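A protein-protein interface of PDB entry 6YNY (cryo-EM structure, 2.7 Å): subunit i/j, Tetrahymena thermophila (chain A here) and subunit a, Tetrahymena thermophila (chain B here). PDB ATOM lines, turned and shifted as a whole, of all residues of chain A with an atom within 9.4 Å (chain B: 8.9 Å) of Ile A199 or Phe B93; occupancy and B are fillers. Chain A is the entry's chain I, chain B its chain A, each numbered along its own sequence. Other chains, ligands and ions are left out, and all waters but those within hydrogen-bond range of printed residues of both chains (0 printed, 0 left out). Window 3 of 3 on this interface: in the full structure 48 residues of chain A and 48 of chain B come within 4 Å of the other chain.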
ATOM      1  N   ARG A 172     -16.067   9.084   7.074  1.00  0.00           N
ATOM      2  CA  ARG A 172     -15.925   9.136   8.523  1.00  0.00           C
ATOM      3  C   ARG A 172     -15.732  10.557   9.025  1.00  0.00           C
ATOM      4  O   ARG A 172     -16.128  10.869  10.153  1.00  0.00           O
ATOM      5  CB  ARG A 172     -14.749   8.268   8.965  1.00  0.00           C
ATOM      6  CG  ARG A 172     -14.669   8.059  10.458  1.00  0.00           C
ATOM      7  CD  ARG A 172     -13.465   7.232  10.829  1.00  0.00           C
ATOM      8  NE  ARG A 172     -13.418   6.936  12.255  1.00  0.00           N
ATOM      9  CZ  ARG A 172     -12.918   7.751  13.176  1.00  0.00           C
ATOM     10  NH1 ARG A 172     -12.419   8.928  12.837  1.00  0.00           N
ATOM     11  NH2 ARG A 172     -12.922   7.385  14.446  1.00  0.00           N
ATOM     12  N   SER A 173     -15.131  11.427   8.213  1.00  0.00           N
ATOM     13  CA  SER A 173     -14.952  12.812   8.625  1.00  0.00           C
ATOM     14  C   SER A 173     -16.288  13.512   8.813  1.00  0.00           C
ATOM     15  O   SER A 173     -16.415  14.388   9.676  1.00  0.00           O
ATOM     16  CB  SER A 173     -14.104  13.555   7.595  1.00  0.00           C
ATOM     17  OG  SER A 173     -12.836  12.944   7.453  1.00  0.00           O
ATOM     18  N   ASP A 177     -19.080  12.272  16.526  1.00  0.00           N
ATOM     19  CA  ASP A 177     -18.259  11.574  17.508  1.00  0.00           C
ATOM     20  C   ASP A 177     -18.991  10.378  18.098  1.00  0.00           C
ATOM     21  O   ASP A 177     -18.367   9.361  18.420  1.00  0.00           O
ATOM     22  CB  ASP A 177     -17.847  12.540  18.616  1.00  0.00           C
ATOM     23  CG  ASP A 177     -16.816  11.949  19.554  1.00  0.00           C
ATOM     24  OD1 ASP A 177     -15.640  11.839  19.148  1.00  0.00           O
ATOM     25  OD2 ASP A 177     -17.179  11.596  20.696  1.00  0.00           O
ATOM     26  N   LYS A 180     -18.826   7.437  15.365  1.00  0.00           N
ATOM     27  CA  LYS A 180     -17.507   6.855  15.167  1.00  0.00           C
ATOM     28  C   LYS A 180     -16.953   6.189  16.417  1.00  0.00           C
ATOM     29  O   LYS A 180     -15.878   5.585  16.348  1.00  0.00           O
ATOM     30  CB  LYS A 180     -16.530   7.925  14.679  1.00  0.00           C
ATOM     31  CG  LYS A 180     -16.350   9.078  15.627  1.00  0.00           C
ATOM     32  CD  LYS A 180     -15.282  10.037  15.133  1.00  0.00           C
ATOM     33  CE  LYS A 180     -15.687  10.706  13.841  1.00  0.00           C
ATOM     34  NZ  LYS A 180     -14.764  11.805  13.478  1.00  0.00           N
ATOM     35  N   LYS A 181     -17.643   6.285  17.551  1.00  0.00           N
ATOM     36  CA  LYS A 181     -17.221   5.612  18.767  1.00  0.00           C
ATOM     37  C   LYS A 181     -18.143   4.478  19.185  1.00  0.00           C
ATOM     38  O   LYS A 181     -17.803   3.742  20.117  1.00  0.00           O
ATOM     39  CB  LYS A 181     -17.107   6.618  19.919  1.00  0.00           C
ATOM     40  CG  LYS A 181     -15.956   7.585  19.772  1.00  0.00           C
ATOM     41  CD  LYS A 181     -15.601   8.238  21.088  1.00  0.00           C
ATOM     42  CE  LYS A 181     -14.485   9.246  20.926  1.00  0.00           C
ATOM     43  NZ  LYS A 181     -13.295   8.654  20.265  1.00  0.00           N
ATOM     44  N   LEU A 194     -16.751  12.899  25.342  1.00  0.00           N
ATOM     45  CA  LEU A 194     -15.507  13.505  25.777  1.00  0.00           C
ATOM     46  C   LEU A 194     -15.491  14.989  25.442  1.00  0.00           C
ATOM     47  O   LEU A 194     -16.192  15.440  24.530  1.00  0.00           O
ATOM     48  CB  LEU A 194     -14.309  12.824  25.104  1.00  0.00           C
ATOM     49  CG  LEU A 194     -13.810  11.528  25.734  1.00  0.00           C
ATOM     50  CD1 LEU A 194     -13.062  10.705  24.718  1.00  0.00           C
ATOM     51  CD2 LEU A 194     -12.912  11.832  26.913  1.00  0.00           C
ATOM     52  N   PRO A 195     -14.703  15.784  26.163  1.00  0.00           N
ATOM     53  CA  PRO A 195     -14.594  17.205  25.822  1.00  0.00           C
ATOM     54  C   PRO A 195     -14.105  17.400  24.396  1.00  0.00           C
ATOM     55  O   PRO A 195     -13.207  16.700  23.924  1.00  0.00           O
ATOM     56  CB  PRO A 195     -13.584  17.738  26.842  1.00  0.00           C
ATOM     57  CG  PRO A 195     -13.650  16.789  27.972  1.00  0.00           C
ATOM     58  CD  PRO A 195     -13.957  15.454  27.388  1.00  0.00           C
ATOM     59  N   VAL A 196     -14.711  18.367  23.711  1.00  0.00           N
ATOM     60  CA  VAL A 196     -14.359  18.640  22.324  1.00  0.00           C
ATOM     61  C   VAL A 196     -13.004  19.329  22.270  1.00  0.00           C
ATOM     62  O   VAL A 196     -12.732  20.263  23.035  1.00  0.00           O
ATOM     63  CB  VAL A 196     -15.447  19.492  21.654  1.00  0.00           C
ATOM     64  CG1 VAL A 196     -15.085  19.776  20.211  1.00  0.00           C
ATOM     65  CG2 VAL A 196     -16.784  18.791  21.736  1.00  0.00           C
ATOM     66  N   VAL A 197     -12.144  18.865  21.363  1.00  0.00           N
ATOM     67  CA  VAL A 197     -10.823  19.441  21.163  1.00  0.00           C
ATOM     68  C   VAL A 197     -10.567  19.563  19.668  1.00  0.00           C
ATOM     69  O   VAL A 197     -11.233  18.932  18.845  1.00  0.00           O
ATOM     70  CB  VAL A 197      -9.709  18.606  21.829  1.00  0.00           C
ATOM     71  CG1 VAL A 197      -9.846  18.652  23.334  1.00  0.00           C
ATOM     72  CG2 VAL A 197      -9.754  17.174  21.338  1.00  0.00           C
ATOM     73  N   SER A 198      -9.580  20.385  19.325  1.00  0.00           N
ATOM     74  CA  SER A 198      -9.217  20.631  17.934  1.00  0.00           C
ATOM     75  C   SER A 198      -8.155  19.625  17.514  1.00  0.00           C
ATOM     76  O   SER A 198      -6.994  19.725  17.925  1.00  0.00           O
ATOM     77  CB  SER A 198      -8.715  22.060  17.753  1.00  0.00           C
ATOM     78  OG  SER A 198      -9.714  23.002  18.101  1.00  0.00           O
ATOM     79  N   ILE A 199      -8.553  18.656  16.697  1.00  0.00           N
ATOM     80  CA  ILE A 199      -7.634  17.651  16.172  1.00  0.00           C
ATOM     81  C   ILE A 199      -7.810  17.608  14.659  1.00  0.00           C
ATOM     82  O   ILE A 199      -8.830  17.102  14.172  1.00  0.00           O
ATOM     83  CB  ILE A 199      -7.885  16.278  16.810  1.00  0.00           C
ATOM     84  CG1 ILE A 199      -7.621  16.348  18.312  1.00  0.00           C
ATOM     85  CG2 ILE A 199      -6.998  15.235  16.173  1.00  0.00           C
ATOM     86  CD1 ILE A 199      -8.052  15.130  19.067  1.00  0.00           C
ATOM     87  N   PRO A 200      -6.856  18.118  13.881  1.00  0.00           N
ATOM     88  CA  PRO A 200      -7.048  18.176  12.429  1.00  0.00           C
ATOM     89  C   PRO A 200      -7.258  16.800  11.818  1.00  0.00           C
ATOM     90  O   PRO A 200      -6.902  15.768  12.389  1.00  0.00           O
ATOM     91  CB  PRO A 200      -5.746  18.809  11.924  1.00  0.00           C
ATOM     92  CG  PRO A 200      -5.182  19.519  13.090  1.00  0.00           C
ATOM     93  CD  PRO A 200      -5.580  18.730  14.287  1.00  0.00           C
ATOM     94  N   ASN A 201      -7.853  16.805  10.631  1.00  0.00           N
ATOM     95  CA  ASN A 201      -8.050  15.604   9.826  1.00  0.00           C
ATOM     96  C   ASN A 201      -7.092  15.702   8.643  1.00  0.00           C
ATOM     97  O   ASN A 201      -7.448  16.204   7.576  1.00  0.00           O
ATOM     98  CB  ASN A 201      -9.494  15.477   9.363  1.00  0.00           C
ATOM     99  CG  ASN A 201      -9.696  14.322   8.403  1.00  0.00           C
ATOM    100  OD1 ASN A 201      -8.957  13.340   8.432  1.00  0.00           O
ATOM    101  ND2 ASN A 201     -10.696  14.440   7.538  1.00  0.00           N
ATOM    102  N   VAL A 202      -5.871  15.218   8.840  1.00  0.00           N
ATOM    103  CA  VAL A 202      -4.836  15.229   7.815  1.00  0.00           C
ATOM    104  C   VAL A 202      -4.668  13.804   7.312  1.00  0.00           C
ATOM    105  O   VAL A 202      -4.420  12.883   8.099  1.00  0.00           O
ATOM    106  CB  VAL A 202      -3.512  15.797   8.349  1.00  0.00           C
ATOM    107  CG1 VAL A 202      -2.982  14.958   9.496  1.00  0.00           C
ATOM    108  CG2 VAL A 202      -2.485  15.882   7.233  1.00  0.00           C
ATOM    109  N   LEU A 203      -4.810  13.621   5.999  1.00  0.00           N
ATOM    110  CA  LEU A 203      -4.704  12.287   5.422  1.00  0.00           C
ATOM    111  C   LEU A 203      -3.284  11.752   5.544  1.00  0.00           C
ATOM    112  O   LEU A 203      -3.052  10.696   6.143  1.00  0.00           O
ATOM    113  CB  LEU A 203      -5.139  12.314   3.960  1.00  0.00           C
ATOM    114  CG  LEU A 203      -6.544  12.841   3.685  1.00  0.00           C
ATOM    115  CD1 LEU A 203      -6.823  12.838   2.197  1.00  0.00           C
ATOM    116  CD2 LEU A 203      -7.567  12.003   4.419  1.00  0.00           C
ATOM    117  N   ASN A 204      -2.319  12.472   4.979  1.00  0.00           N
ATOM    118  CA  ASN A 204      -0.927  12.054   4.982  1.00  0.00           C
ATOM    119  C   ASN A 204      -0.090  13.119   5.676  1.00  0.00           C
ATOM    120  O   ASN A 204      -0.031  14.261   5.188  1.00  0.00           O
ATOM    121  CB  ASN A 204      -0.433  11.831   3.555  1.00  0.00           C
ATOM    122  CG  ASN A 204       0.712  10.850   3.483  1.00  0.00           C
ATOM    123  OD1 ASN A 204       0.509   9.654   3.278  1.00  0.00           O
ATOM    124  ND2 ASN A 204       1.922  11.349   3.650  1.00  0.00           N
ATOM    125  N   PRO A 205       0.563  12.817   6.801  1.00  0.00           N
ATOM    126  CA  PRO A 205       1.417  13.835   7.433  1.00  0.00           C
ATOM    127  C   PRO A 205       2.444  14.397   6.475  1.00  0.00           C
ATOM    128  O   PRO A 205       2.609  15.618   6.372  1.00  0.00           O
ATOM    129  CB  PRO A 205       2.064  13.070   8.590  1.00  0.00           C
ATOM    130  CG  PRO A 205       1.156  11.945   8.864  1.00  0.00           C
ATOM    131  CD  PRO A 205       0.577  11.553   7.551  1.00  0.00           C
ATOM    132  N   TYR B  83       9.188   9.319   9.225  1.00  0.00           N
ATOM    133  CA  TYR B  83       8.317   9.375  10.390  1.00  0.00           C
ATOM    134  C   TYR B  83       9.092   9.591  11.678  1.00  0.00           C
ATOM    135  O   TYR B  83       8.515  10.065  12.659  1.00  0.00           O
ATOM    136  CB  TYR B  83       7.489   8.098  10.487  1.00  0.00           C
ATOM    137  CG  TYR B  83       6.158   8.188   9.791  1.00  0.00           C
ATOM    138  CD1 TYR B  83       4.976   8.159  10.510  1.00  0.00           C
ATOM    139  CD2 TYR B  83       6.082   8.322   8.419  1.00  0.00           C
ATOM    140  CE1 TYR B  83       3.761   8.247   9.881  1.00  0.00           C
ATOM    141  CE2 TYR B  83       4.872   8.412   7.780  1.00  0.00           C
ATOM    142  CZ  TYR B  83       3.713   8.374   8.515  1.00  0.00           C
ATOM    143  OH  TYR B  83       2.501   8.465   7.874  1.00  0.00           O
ATOM    144  N   LEU B  86       9.673  13.245  11.479  1.00  0.00           N
ATOM    145  CA  LEU B  86       8.358  13.837  11.671  1.00  0.00           C
ATOM    146  C   LEU B  86       7.975  13.876  13.143  1.00  0.00           C
ATOM    147  O   LEU B  86       7.305  14.815  13.585  1.00  0.00           O
ATOM    148  CB  LEU B  86       7.332  13.047  10.870  1.00  0.00           C
ATOM    149  CG  LEU B  86       5.902  13.562  10.832  1.00  0.00           C
ATOM    150  CD1 LEU B  86       5.840  14.902  10.151  1.00  0.00           C
ATOM    151  CD2 LEU B  86       5.039  12.560  10.112  1.00  0.00           C
ATOM    152  N   SER B  87       8.384  12.868  13.914  1.00  0.00           N
ATOM    153  CA  SER B  87       8.084  12.825  15.335  1.00  0.00           C
ATOM    154  C   SER B  87       8.943  13.779  16.150  1.00  0.00           C
ATOM    155  O   SER B  87       8.607  14.058  17.305  1.00  0.00           O
ATOM    156  CB  SER B  87       8.271  11.403  15.863  1.00  0.00           C
ATOM    157  OG  SER B  87       9.624  11.001  15.770  1.00  0.00           O
ATOM    158  N   LEU B  88      10.041  14.279  15.585  1.00  0.00           N
ATOM    159  CA  LEU B  88      10.893  15.201  16.323  1.00  0.00           C
ATOM    160  C   LEU B  88      10.272  16.585  16.415  1.00  0.00           C
ATOM    161  O   LEU B  88      10.526  17.310  17.383  1.00  0.00           O
ATOM    162  CB  LEU B  88      12.267  15.295  15.660  1.00  0.00           C
ATOM    163  CG  LEU B  88      13.019  13.985  15.456  1.00  0.00           C
ATOM    164  CD1 LEU B  88      14.362  14.243  14.816  1.00  0.00           C
ATOM    165  CD2 LEU B  88      13.186  13.250  16.757  1.00  0.00           C
ATOM    166  N   SER B  89       9.468  16.962  15.429  1.00  0.00           N
ATOM    167  CA  SER B  89       8.833  18.268  15.421  1.00  0.00           C
ATOM    168  C   SER B  89       7.554  18.238  16.243  1.00  0.00           C
ATOM    169  O   SER B  89       6.808  17.256  16.225  1.00  0.00           O
ATOM    170  CB  SER B  89       8.528  18.704  13.990  1.00  0.00           C
ATOM    171  OG  SER B  89       7.668  17.780  13.348  1.00  0.00           O
ATOM    172  N   THR B  90       7.308  19.324  16.967  1.00  0.00           N
ATOM    173  CA  THR B  90       6.130  19.407  17.816  1.00  0.00           C
ATOM    174  C   THR B  90       4.869  19.310  16.972  1.00  0.00           C
ATOM    175  O   THR B  90       4.680  20.080  16.026  1.00  0.00           O
ATOM    176  CB  THR B  90       6.141  20.710  18.606  1.00  0.00           C
ATOM    177  OG1 THR B  90       7.393  20.846  19.290  1.00  0.00           O
ATOM    178  CG2 THR B  90       5.019  20.718  19.619  1.00  0.00           C
ATOM    179  N   SER B  91       4.009  18.357  17.317  1.00  0.00           N
ATOM    180  CA  SER B  91       2.757  18.152  16.611  1.00  0.00           C
ATOM    181  C   SER B  91       1.758  17.525  17.569  1.00  0.00           C
ATOM    182  O   SER B  91       2.114  17.050  18.650  1.00  0.00           O
ATOM    183  CB  SER B  91       2.947  17.273  15.375  1.00  0.00           C
ATOM    184  OG  SER B  91       1.719  17.056  14.710  1.00  0.00           O
ATOM    185  N   VAL B  92       0.491  17.531  17.158  1.00  0.00           N
ATOM    186  CA  VAL B  92      -0.548  16.918  17.972  1.00  0.00           C
ATOM    187  C   VAL B  92      -0.510  15.401  17.878  1.00  0.00           C
ATOM    188  O   VAL B  92      -0.984  14.719  18.795  1.00  0.00           O
ATOM    189  CB  VAL B  92      -1.930  17.454  17.561  1.00  0.00           C
ATOM    190  CG1 VAL B  92      -2.328  16.923  16.209  1.00  0.00           C
ATOM    191  CG2 VAL B  92      -2.962  17.090  18.589  1.00  0.00           C
ATOM    192  N   PHE B  93       0.044  14.853  16.798  1.00  0.00           N
ATOM    193  CA  PHE B  93       0.184  13.417  16.616  1.00  0.00           C
ATOM    194  C   PHE B  93       1.579  12.924  16.976  1.00  0.00           C
ATOM    195  O   PHE B  93       1.979  11.841  16.537  1.00  0.00           O
ATOM    196  CB  PHE B  93      -0.135  13.032  15.175  1.00  0.00           C
ATOM    197  CG  PHE B  93      -1.487  13.471  14.707  1.00  0.00           C
ATOM    198  CD1 PHE B  93      -2.623  12.773  15.067  1.00  0.00           C
ATOM    199  CD2 PHE B  93      -1.620  14.567  13.882  1.00  0.00           C
ATOM    200  CE1 PHE B  93      -3.863  13.175  14.626  1.00  0.00           C
ATOM    201  CE2 PHE B  93      -2.858  14.969  13.438  1.00  0.00           C
ATOM    202  CZ  PHE B  93      -3.980  14.271  13.811  1.00  0.00           C
ATOM    203  N   GLN B  94       2.325  13.694  17.765  1.00  0.00           N
ATOM    204  CA  GLN B  94       3.710  13.344  18.052  1.00  0.00           C
ATOM    205  C   GLN B  94       3.814  11.985  18.730  1.00  0.00           C
ATOM    206  O   GLN B  94       4.729  11.208  18.441  1.00  0.00           O
ATOM    207  CB  GLN B  94       4.343  14.430  18.916  1.00  0.00           C
ATOM    208  CG  GLN B  94       5.836  14.322  19.055  1.00  0.00           C
ATOM    209  CD  GLN B  94       6.437  15.517  19.757  1.00  0.00           C
ATOM    210  OE1 GLN B  94       5.819  16.111  20.638  1.00  0.00           O
ATOM    211  NE2 GLN B  94       7.646  15.883  19.362  1.00  0.00           N
ATOM    212  N   LEU B  95       2.887  11.681  19.638  1.00  0.00           N
ATOM    213  CA  LEU B  95       2.899  10.383  20.298  1.00  0.00           C
ATOM    214  C   LEU B  95       2.350   9.282  19.403  1.00  0.00           C
ATOM    215  O   LEU B  95       2.752   8.122  19.538  1.00  0.00           O
ATOM    216  CB  LEU B  95       2.092  10.448  21.592  1.00  0.00           C
ATOM    217  CG  LEU B  95       2.002   9.148  22.385  1.00  0.00           C
ATOM    218  CD1 LEU B  95       3.374   8.675  22.803  1.00  0.00           C
ATOM    219  CD2 LEU B  95       1.121   9.333  23.589  1.00  0.00           C
ATOM    220  N   PHE B  96       1.436   9.619  18.497  1.00  0.00           N
ATOM    221  CA  PHE B  96       0.901   8.621  17.581  1.00  0.00           C
ATOM    222  C   PHE B  96       1.978   8.096  16.642  1.00  0.00           C
ATOM    223  O   PHE B  96       2.054   6.890  16.388  1.00  0.00           O
ATOM    224  CB  PHE B  96      -0.258   9.217  16.787  1.00  0.00           C
ATOM    225  CG  PHE B  96      -0.785   8.316  15.723  1.00  0.00           C
ATOM    226  CD1 PHE B  96      -1.503   7.186  16.051  1.00  0.00           C
ATOM    227  CD2 PHE B  96      -0.569   8.602  14.393  1.00  0.00           C
ATOM    228  CE1 PHE B  96      -1.988   6.359  15.075  1.00  0.00           C
ATOM    229  CE2 PHE B  96      -1.055   7.776  13.413  1.00  0.00           C
ATOM    230  CZ  PHE B  96      -1.766   6.655  13.754  1.00  0.00           C
ATOM    231  N   TYR B  97       2.816   8.987  16.114  1.00  0.00           N
ATOM    232  CA  TYR B  97       3.880   8.558  15.215  1.00  0.00           C
ATOM    233  C   TYR B  97       4.872   7.646  15.920  1.00  0.00           C
ATOM    234  O   TYR B  97       5.453   6.757  15.289  1.00  0.00           O
ATOM    235  CB  TYR B  97       4.593   9.778  14.641  1.00  0.00           C
ATOM    236  CG  TYR B  97       3.708  10.695  13.833  1.00  0.00           C
ATOM    237  CD1 TYR B  97       2.654  10.197  13.085  1.00  0.00           C
ATOM    238  CD2 TYR B  97       3.928  12.059  13.818  1.00  0.00           C
ATOM    239  CE1 TYR B  97       1.849  11.031  12.349  1.00  0.00           C
ATOM    240  CE2 TYR B  97       3.128  12.900  13.086  1.00  0.00           C
ATOM    241  CZ  TYR B  97       2.090  12.382  12.353  1.00  0.00           C
ATOM    242  OH  TYR B  97       1.290  13.220  11.617  1.00  0.00           O
ATOM    243  N   ALA B  98       5.078   7.848  17.218  1.00  0.00           N
ATOM    244  CA  ALA B  98       5.971   6.981  17.974  1.00  0.00           C
ATOM    245  C   ALA B  98       5.432   5.560  18.041  1.00  0.00           C
ATOM    246  O   ALA B  98       6.171   4.591  17.834  1.00  0.00           O
ATOM    247  CB  ALA B  98       6.164   7.546  19.375  1.00  0.00           C
ATOM    248  N   VAL B  99       4.141   5.418  18.334  1.00  0.00           N
ATOM    249  CA  VAL B  99       3.521   4.099  18.369  1.00  0.00           C
ATOM    250  C   VAL B  99       3.628   3.426  17.009  1.00  0.00           C
ATOM    251  O   VAL B  99       3.831   2.210  16.913  1.00  0.00           O
ATOM    252  CB  VAL B  99       2.059   4.224  18.830  1.00  0.00           C
ATOM    253  CG1 VAL B  99       1.360   2.894  18.764  1.00  0.00           C
ATOM    254  CG2 VAL B  99       1.998   4.781  20.233  1.00  0.00           C
ATOM    255  N   ILE B 100       3.497   4.203  15.935  1.00  0.00           N
ATOM    256  CA  ILE B 100       3.618   3.652  14.590  1.00  0.00           C
ATOM    257  C   ILE B 100       5.015   3.093  14.365  1.00  0.00           C
ATOM    258  O   ILE B 100       5.184   1.979  13.857  1.00  0.00           O
ATOM    259  CB  ILE B 100       3.271   4.726  13.547  1.00  0.00           C
ATOM    260  CG1 ILE B 100       1.791   5.083  13.624  1.00  0.00           C
ATOM    261  CG2 ILE B 100       3.643   4.261  12.166  1.00  0.00           C
ATOM    262  CD1 ILE B 100       0.867   3.953  13.303  1.00  0.00           C
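The side-chain hydroxyl of Ser B91 lies close to the backbone NH of Phe B93 (3.5 Å).
The backbone carbonyl oxygen of Tyr B83 is in hydrogen-bond range of the side-chain hydroxyl of Ser B87, at 3.4 Å.
The backbone carbonyl oxygen (O) of Leu B86 is in hydrogen-bond range of the side-chain hydroxyl (OG) of Ser B89, at 3.0 Å.
Ile A199 touches Phe B93.
O of Pro A200 touches CZ of Phe B93, at 3.6 Å.
Phe B93 touches Val A202 (CE2 to CG1, 3.9 Å).
Pro A205 touches Tyr B83 (CD to OH, 3.7 Å).
Pro A205 touches Leu B86.
Pro A205 touches Tyr B97 (CG to OH, 3.0 Å).
No residue of chain B comes within 4 Å of Ser A198.
Of the printed residues of chain B, Ile A199 touches Phe B93.
Of the printed residues of chain B, Val A202 touches Phe B93 (3.9 Å).
Of the printed residues of chain B, Pro A205 touches Tyr B83, Leu B86 and Tyr B97.
No residue of chain A comes within 4 Å of Ser B91.
No residue of chain A comes within 4 Å of Val B92.
Of the printed residues of chain A, Phe B93 touches Ile A199, Pro A200 and Val A202.
Printed residues of chain A within 4 Å of Tyr B97: Pro A205.
The nearest residue of chain B that does not touch Ile A199 is Val B92 (4.7 Å).
Printed residues of chain A that touch a printed residue of chain B: Ile A199, Pro A200, Val A202 and Pro A205.
Hydrophobic or aromatic side chains of chain B that line the printed part of chain A: Tyr B83, Leu B86, Phe B93 and Tyr B97.
Among the printed residues, no Asp or Glu carboxylate lies within 4 Å of a Lys or Arg side-chain nitrogen of the other chain.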
